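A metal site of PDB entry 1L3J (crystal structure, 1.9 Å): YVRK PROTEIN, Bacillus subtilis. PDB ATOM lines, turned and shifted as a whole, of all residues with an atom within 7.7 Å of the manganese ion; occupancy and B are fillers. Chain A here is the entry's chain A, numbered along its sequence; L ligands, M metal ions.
Of the 21 residues printed, 4 come within 4 Å of the manganese ion. The nearest printed residue that does not touch the manganese ion is Phe 155 (4.3 Å).
N of Phe 134 sits at hydrogen-bond distance from O of Glu 101, 2.7 Å away. OE2 of Glu 101 sits at hydrogen-bond distance from NE1 of Trp 132 (3.0 Å). A ring nitrogen (ND1) of His 95 lies within hydrogen-bond range of the guanidinium group (NH1) of Arg 92 (3.4 Å). O of Glu 93 is in hydrogen-bond range of ND1 of His 95 (2.6 Å). ND1 of His 140 sits at hydrogen-bond distance from O of Leu 138 (2.9 Å). A ring nitrogen (ND1) of His 97 lies within hydrogen-bond range of the backbone carbonyl oxygen (O) of Glu 99, at 3.5 Å.
The side-chain carboxylate (OE1) of Glu 101 is bound to the manganese ion (2.0 Å). O2 of the ligand is bound to the manganese ion (2.1 Å). A ring nitrogen (NE2) of His 95 is bound to the manganese ion. The manganese ion is bound by NE2 of His 140, 2.2 Å away. NE2 of His 97 binds the manganese ion (2.2 Å).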
ATOM      1  N   MET A  84     -19.173  28.369  -6.701  1.00  0.00           N
ATOM      2  CA  MET A  84     -19.932  29.431  -7.372  1.00  0.00           C
ATOM      3  C   MET A  84     -20.531  30.412  -6.372  1.00  0.00           C
ATOM      4  O   MET A  84     -20.960  30.033  -5.286  1.00  0.00           O
ATOM      5  CB  MET A  84     -21.040  28.801  -8.245  1.00  0.00           C
ATOM      6  CG  MET A  84     -21.879  29.807  -9.047  1.00  0.00           C
ATOM      7  SD  MET A  84     -22.897  29.032 -10.360  1.00  0.00           S
ATOM      8  CE  MET A  84     -21.626  28.796 -11.649  1.00  0.00           C
ATOM      9  N   ARG A  92     -27.880  31.956 -12.763  1.00  0.00           N
ATOM     10  CA  ARG A  92     -26.902  31.116 -13.431  1.00  0.00           C
ATOM     11  C   ARG A  92     -27.782  30.602 -14.572  1.00  0.00           C
ATOM     12  O   ARG A  92     -28.719  29.831 -14.346  1.00  0.00           O
ATOM     13  CB  ARG A  92     -26.446  29.958 -12.544  1.00  0.00           C
ATOM     14  CG  ARG A  92     -25.670  28.875 -13.293  1.00  0.00           C
ATOM     15  CD  ARG A  92     -24.368  29.398 -13.910  1.00  0.00           C
ATOM     16  NE  ARG A  92     -23.656  28.339 -14.631  1.00  0.00           N
ATOM     17  CZ  ARG A  92     -23.860  28.006 -15.901  1.00  0.00           C
ATOM     18  NH1 ARG A  92     -24.766  28.661 -16.622  1.00  0.00           N
ATOM     19  NH2 ARG A  92     -23.175  27.013 -16.441  1.00  0.00           N
ATOM     20  N   GLU A  93     -27.498  31.075 -15.775  1.00  0.00           N
ATOM     21  CA  GLU A  93     -28.279  30.742 -16.972  1.00  0.00           C
ATOM     22  C   GLU A  93     -28.711  29.292 -17.163  1.00  0.00           C
ATOM     23  O   GLU A  93     -27.945  28.362 -16.916  1.00  0.00           O
ATOM     24  CB  GLU A  93     -27.509  31.186 -18.219  1.00  0.00           C
ATOM     25  CG  GLU A  93     -28.291  30.948 -19.498  1.00  0.00           C
ATOM     26  CD  GLU A  93     -27.528  31.316 -20.739  1.00  0.00           C
ATOM     27  OE1 GLU A  93     -26.444  31.941 -20.636  1.00  0.00           O
ATOM     28  OE2 GLU A  93     -28.019  30.984 -21.836  1.00  0.00           O
ATOM     29  N   HIS A  95     -29.207  25.814 -18.319  1.00  0.00           N
ATOM     30  CA  HIS A  95     -28.193  25.015 -19.006  1.00  0.00           C
ATOM     31  C   HIS A  95     -28.295  23.541 -18.647  1.00  0.00           C
ATOM     32  O   HIS A  95     -29.139  23.140 -17.836  1.00  0.00           O
ATOM     33  CB  HIS A  95     -26.805  25.510 -18.600  1.00  0.00           C
ATOM     34  CG  HIS A  95     -26.474  25.246 -17.156  1.00  0.00           C
ATOM     35  ND1 HIS A  95     -26.900  26.059 -16.126  1.00  0.00           N
ATOM     36  CD2 HIS A  95     -25.804  24.225 -16.571  1.00  0.00           C
ATOM     37  CE1 HIS A  95     -26.511  25.547 -14.968  1.00  0.00           C
ATOM     38  NE2 HIS A  95     -25.843  24.437 -15.213  1.00  0.00           N
ATOM     39  N   TRP A  96     -27.425  22.739 -19.252  1.00  0.00           N
ATOM     40  CA  TRP A  96     -27.383  21.310 -18.947  1.00  0.00           C
ATOM     41  C   TRP A  96     -25.963  20.825 -19.254  1.00  0.00           C
ATOM     42  O   TRP A  96     -25.193  21.524 -19.898  1.00  0.00           O
ATOM     43  CB  TRP A  96     -28.432  20.539 -19.769  1.00  0.00           C
ATOM     44  CG  TRP A  96     -28.118  20.334 -21.247  1.00  0.00           C
ATOM     45  CD1 TRP A  96     -27.498  19.251 -21.815  1.00  0.00           C
ATOM     46  CD2 TRP A  96     -28.448  21.211 -22.327  1.00  0.00           C
ATOM     47  NE1 TRP A  96     -27.427  19.402 -23.175  1.00  0.00           N
ATOM     48  CE2 TRP A  96     -28.001  20.593 -23.517  1.00  0.00           C
ATOM     49  CE3 TRP A  96     -29.081  22.461 -22.418  1.00  0.00           C
ATOM     50  CZ2 TRP A  96     -28.165  21.179 -24.783  1.00  0.00           C
ATOM     51  CZ3 TRP A  96     -29.239  23.048 -23.671  1.00  0.00           C
ATOM     52  CH2 TRP A  96     -28.786  22.407 -24.840  1.00  0.00           C
ATOM     53  N   HIS A  97     -25.597  19.663 -18.723  1.00  0.00           N
ATOM     54  CA  HIS A  97     -24.272  19.112 -19.006  1.00  0.00           C
ATOM     55  C   HIS A  97     -24.320  17.607 -19.084  1.00  0.00           C
ATOM     56  O   HIS A  97     -25.325  16.985 -18.756  1.00  0.00           O
ATOM     57  CB  HIS A  97     -23.205  19.525 -17.978  1.00  0.00           C
ATOM     58  CG  HIS A  97     -23.720  20.294 -16.803  1.00  0.00           C
ATOM     59  ND1 HIS A  97     -24.496  19.729 -15.819  1.00  0.00           N
ATOM     60  CD2 HIS A  97     -23.530  21.587 -16.428  1.00  0.00           C
ATOM     61  CE1 HIS A  97     -24.754  20.628 -14.887  1.00  0.00           C
ATOM     62  NE2 HIS A  97     -24.183  21.763 -15.244  1.00  0.00           N
ATOM     63  N   GLU A  99     -22.472  15.676 -17.313  1.00  0.00           N
ATOM     64  CA  GLU A  99     -22.267  15.141 -15.975  1.00  0.00           C
ATOM     65  C   GLU A  99     -23.424  15.398 -15.013  1.00  0.00           C
ATOM     66  O   GLU A  99     -24.205  16.333 -15.191  1.00  0.00           O
ATOM     67  CB  GLU A  99     -20.996  15.734 -15.364  1.00  0.00           C
ATOM     68  CG  GLU A  99     -19.745  15.518 -16.223  1.00  0.00           C
ATOM     69  CD  GLU A  99     -19.513  16.623 -17.232  1.00  0.00           C
ATOM     70  OE1 GLU A  99     -20.470  17.345 -17.582  1.00  0.00           O
ATOM     71  OE2 GLU A  99     -18.357  16.761 -17.691  1.00  0.00           O
ATOM     72  N   ALA A 100     -23.538  14.540 -14.002  1.00  0.00           N
ATOM     73  CA  ALA A 100     -24.560  14.727 -12.974  1.00  0.00           C
ATOM     74  C   ALA A 100     -23.977  15.824 -12.085  1.00  0.00           C
ATOM     75  O   ALA A 100     -22.755  15.989 -12.006  1.00  0.00           O
ATOM     76  CB  ALA A 100     -24.754  13.443 -12.176  1.00  0.00           C
ATOM     77  N   GLU A 101     -24.856  16.568 -11.418  1.00  0.00           N
ATOM     78  CA  GLU A 101     -24.430  17.675 -10.558  1.00  0.00           C
ATOM     79  C   GLU A 101     -25.003  17.562  -9.161  1.00  0.00           C
ATOM     80  O   GLU A 101     -26.199  17.363  -8.993  1.00  0.00           O
ATOM     81  CB  GLU A 101     -24.881  18.998 -11.183  1.00  0.00           C
ATOM     82  CG  GLU A 101     -24.597  20.244 -10.357  1.00  0.00           C
ATOM     83  CD  GLU A 101     -25.120  21.498 -11.031  1.00  0.00           C
ATOM     84  OE1 GLU A 101     -24.846  21.680 -12.237  1.00  0.00           O
ATOM     85  OE2 GLU A 101     -25.811  22.310 -10.362  1.00  0.00           O
ATOM     86  N   TRP A 132     -28.817  19.622  -3.600  1.00  0.00           N
ATOM     87  CA  TRP A 132     -29.600  19.362  -4.799  1.00  0.00           C
ATOM     88  C   TRP A 132     -28.770  18.412  -5.635  1.00  0.00           C
ATOM     89  O   TRP A 132     -27.549  18.311  -5.472  1.00  0.00           O
ATOM     90  CB  TRP A 132     -29.969  20.653  -5.562  1.00  0.00           C
ATOM     91  CG  TRP A 132     -28.898  21.379  -6.309  1.00  0.00           C
ATOM     92  CD1 TRP A 132     -28.149  20.915  -7.343  1.00  0.00           C
ATOM     93  CD2 TRP A 132     -28.534  22.759  -6.137  1.00  0.00           C
ATOM     94  NE1 TRP A 132     -27.338  21.917  -7.843  1.00  0.00           N
ATOM     95  CE2 TRP A 132     -27.564  23.055  -7.118  1.00  0.00           C
ATOM     96  CE3 TRP A 132     -28.947  23.766  -5.264  1.00  0.00           C
ATOM     97  CZ2 TRP A 132     -26.992  24.333  -7.233  1.00  0.00           C
ATOM     98  CZ3 TRP A 132     -28.380  25.028  -5.375  1.00  0.00           C
ATOM     99  CH2 TRP A 132     -27.403  25.297  -6.359  1.00  0.00           C
ATOM    100  N   PHE A 134     -28.793  17.075  -9.747  1.00  0.00           N
ATOM    101  CA  PHE A 134     -29.393  17.113 -11.062  1.00  0.00           C
ATOM    102  C   PHE A 134     -28.792  16.018 -11.917  1.00  0.00           C
ATOM    103  O   PHE A 134     -27.596  16.066 -12.233  1.00  0.00           O
ATOM    104  CB  PHE A 134     -29.150  18.474 -11.731  1.00  0.00           C
ATOM    105  CG  PHE A 134     -29.628  19.645 -10.930  1.00  0.00           C
ATOM    106  CD1 PHE A 134     -30.805  19.568 -10.183  1.00  0.00           C
ATOM    107  CD2 PHE A 134     -28.926  20.849 -10.944  1.00  0.00           C
ATOM    108  CE1 PHE A 134     -31.287  20.679  -9.479  1.00  0.00           C
ATOM    109  CE2 PHE A 134     -29.400  21.964 -10.244  1.00  0.00           C
ATOM    110  CZ  PHE A 134     -30.578  21.872  -9.511  1.00  0.00           C
ATOM    111  N   LEU A 138     -30.189  16.668 -17.641  1.00  0.00           N
ATOM    112  CA  LEU A 138     -31.445  17.371 -17.351  1.00  0.00           C
ATOM    113  C   LEU A 138     -31.177  18.863 -17.163  1.00  0.00           C
ATOM    114  O   LEU A 138     -30.326  19.247 -16.362  1.00  0.00           O
ATOM    115  CB  LEU A 138     -32.122  16.769 -16.114  1.00  0.00           C
ATOM    116  CG  LEU A 138     -32.487  15.290 -16.257  1.00  0.00           C
ATOM    117  CD1 LEU A 138     -33.339  14.848 -15.058  1.00  0.00           C
ATOM    118  CD2 LEU A 138     -33.262  15.070 -17.556  1.00  0.00           C
ATOM    119  N   PRO A 139     -31.902  19.718 -17.901  1.00  0.00           N
ATOM    120  CA  PRO A 139     -31.741  21.168 -17.842  1.00  0.00           C
ATOM    121  C   PRO A 139     -32.168  21.810 -16.521  1.00  0.00           C
ATOM    122  O   PRO A 139     -33.207  21.476 -15.950  1.00  0.00           O
ATOM    123  CB  PRO A 139     -32.579  21.650 -19.016  1.00  0.00           C
ATOM    124  CG  PRO A 139     -33.733  20.692 -18.983  1.00  0.00           C
ATOM    125  CD  PRO A 139     -33.036  19.347 -18.776  1.00  0.00           C
ATOM    126  N   HIS A 140     -31.351  22.758 -16.061  1.00  0.00           N
ATOM    127  CA  HIS A 140     -31.626  23.420 -14.797  1.00  0.00           C
ATOM    128  C   HIS A 140     -31.106  24.854 -14.747  1.00  0.00           C
ATOM    129  O   HIS A 140     -30.424  25.327 -15.651  1.00  0.00           O
ATOM    130  CB  HIS A 140     -31.003  22.621 -13.655  1.00  0.00           C
ATOM    131  CG  HIS A 140     -29.557  22.305 -13.866  1.00  0.00           C
ATOM    132  ND1 HIS A 140     -29.127  21.226 -14.610  1.00  0.00           N
ATOM    133  CD2 HIS A 140     -28.431  22.930 -13.438  1.00  0.00           C
ATOM    134  CE1 HIS A 140     -27.812  21.197 -14.635  1.00  0.00           C
ATOM    135  NE2 HIS A 140     -27.360  22.220 -13.923  1.00  0.00           N
ATOM    136  N   SER A 141     -31.435  25.543 -13.646  1.00  0.00           N
ATOM    137  CA  SER A 141     -31.009  26.916 -13.448  1.00  0.00           C
ATOM    138  C   SER A 141     -30.909  27.187 -11.955  1.00  0.00           C
ATOM    139  O   SER A 141     -31.442  26.432 -11.145  1.00  0.00           O
ATOM    140  CB  SER A 141     -32.013  27.889 -14.063  1.00  0.00           C
ATOM    141  OG  SER A 141     -33.247  27.850 -13.362  1.00  0.00           O
ATOM    142  N   ILE A 142     -30.233  28.273 -11.600  1.00  0.00           N
ATOM    143  CA  ILE A 142     -30.085  28.675 -10.207  1.00  0.00           C
ATOM    144  C   ILE A 142     -30.229  30.187 -10.164  1.00  0.00           C
ATOM    145  O   ILE A 142     -29.656  30.889 -10.999  1.00  0.00           O
ATOM    146  CB  ILE A 142     -28.672  28.341  -9.660  1.00  0.00           C
ATOM    147  CG1 ILE A 142     -28.288  26.899  -9.997  1.00  0.00           C
ATOM    148  CG2 ILE A 142     -28.644  28.567  -8.154  1.00  0.00           C
ATOM    149  CD1 ILE A 142     -26.803  26.620  -9.791  1.00  0.00           C
ATOM    150  N   LEU A 153     -20.339  22.972  -5.977  1.00  0.00           N
ATOM    151  CA  LEU A 153     -20.920  22.059  -6.955  1.00  0.00           C
ATOM    152  C   LEU A 153     -19.924  20.921  -7.164  1.00  0.00           C
ATOM    153  O   LEU A 153     -18.714  21.141  -7.168  1.00  0.00           O
ATOM    154  CB  LEU A 153     -21.153  22.770  -8.282  1.00  0.00           C
ATOM    155  CG  LEU A 153     -22.104  23.968  -8.300  1.00  0.00           C
ATOM    156  CD1 LEU A 153     -21.986  24.697  -9.627  1.00  0.00           C
ATOM    157  CD2 LEU A 153     -23.528  23.499  -8.066  1.00  0.00           C
ATOM    158  N   PHE A 155     -19.320  17.604  -9.816  1.00  0.00           N
ATOM    159  CA  PHE A 155     -19.739  16.926 -11.045  1.00  0.00           C
ATOM    160  C   PHE A 155     -19.059  15.568 -11.095  1.00  0.00           C
ATOM    161  O   PHE A 155     -17.879  15.456 -10.740  1.00  0.00           O
ATOM    162  CB  PHE A 155     -19.331  17.780 -12.240  1.00  0.00           C
ATOM    163  CG  PHE A 155     -19.930  19.149 -12.228  1.00  0.00           C
ATOM    164  CD1 PHE A 155     -21.213  19.368 -12.705  1.00  0.00           C
ATOM    165  CD2 PHE A 155     -19.238  20.224 -11.678  1.00  0.00           C
ATOM    166  CE1 PHE A 155     -21.806  20.624 -12.636  1.00  0.00           C
ATOM    167  CE2 PHE A 155     -19.807  21.487 -11.604  1.00  0.00           C
ATOM    168  CZ  PHE A 155     -21.101  21.688 -12.090  1.00  0.00           C
ATOM    169  N   PHE A 160     -14.398  17.539 -16.177  1.00  0.00           N
ATOM    170  CA  PHE A 160     -15.382  18.612 -16.322  1.00  0.00           C
ATOM    171  C   PHE A 160     -14.688  19.883 -16.836  1.00  0.00           C
ATOM    172  O   PHE A 160     -13.664  20.300 -16.280  1.00  0.00           O
ATOM    173  CB  PHE A 160     -16.036  18.893 -14.971  1.00  0.00           C
ATOM    174  CG  PHE A 160     -17.118  19.946 -15.022  1.00  0.00           C
ATOM    175  CD1 PHE A 160     -18.375  19.643 -15.531  1.00  0.00           C
ATOM    176  CD2 PHE A 160     -16.877  21.223 -14.553  1.00  0.00           C
ATOM    177  CE1 PHE A 160     -19.379  20.607 -15.575  1.00  0.00           C
ATOM    178  CE2 PHE A 160     -17.870  22.204 -14.588  1.00  0.00           C
ATOM    179  CZ  PHE A 160     -19.128  21.894 -15.103  1.00  0.00           C
ATOM    180  N   THR A 165     -20.630  21.921 -20.503  1.00  0.00           N
ATOM    181  CA  THR A 165     -21.872  22.680 -20.317  1.00  0.00           C
ATOM    182  C   THR A 165     -22.475  23.352 -21.547  1.00  0.00           C
ATOM    183  O   THR A 165     -21.779  24.017 -22.320  1.00  0.00           O
ATOM    184  CB  THR A 165     -21.673  23.740 -19.216  1.00  0.00           C
ATOM    185  OG1 THR A 165     -21.148  23.110 -18.045  1.00  0.00           O
ATOM    186  CG2 THR A 165     -22.987  24.415 -18.874  1.00  0.00           C
ATOM    187  N   GLN A 167     -25.282  26.066 -22.695  1.00  0.00           N
ATOM    188  CA  GLN A 167     -26.146  27.164 -22.265  1.00  0.00           C
ATOM    189  C   GLN A 167     -27.284  27.406 -23.263  1.00  0.00           C
ATOM    190  O   GLN A 167     -27.074  27.349 -24.474  1.00  0.00           O
ATOM    191  CB  GLN A 167     -25.356  28.469 -22.123  1.00  0.00           C
ATOM    192  CG  GLN A 167     -24.940  28.835 -20.704  1.00  0.00           C
ATOM    193  CD  GLN A 167     -23.838  27.948 -20.163  1.00  0.00           C
ATOM    194  OE1 GLN A 167     -22.763  27.859 -20.752  1.00  0.00           O
ATOM    195  NE2 GLN A 167     -24.091  27.313 -19.028  1.00  0.00           N
HETATM  196  C1  LIG L   1     -23.199  25.152 -12.990  1.00  0.00           C
HETATM  197  O1  LIG L   1     -22.285  25.940 -13.589  1.00  0.00           O
HETATM  198  O2  LIG L   1     -23.488  24.032 -13.383  1.00  0.00           O
HETATM  199 MN    MN M   1     -25.299  22.959 -13.710  1.00  0.00          MN
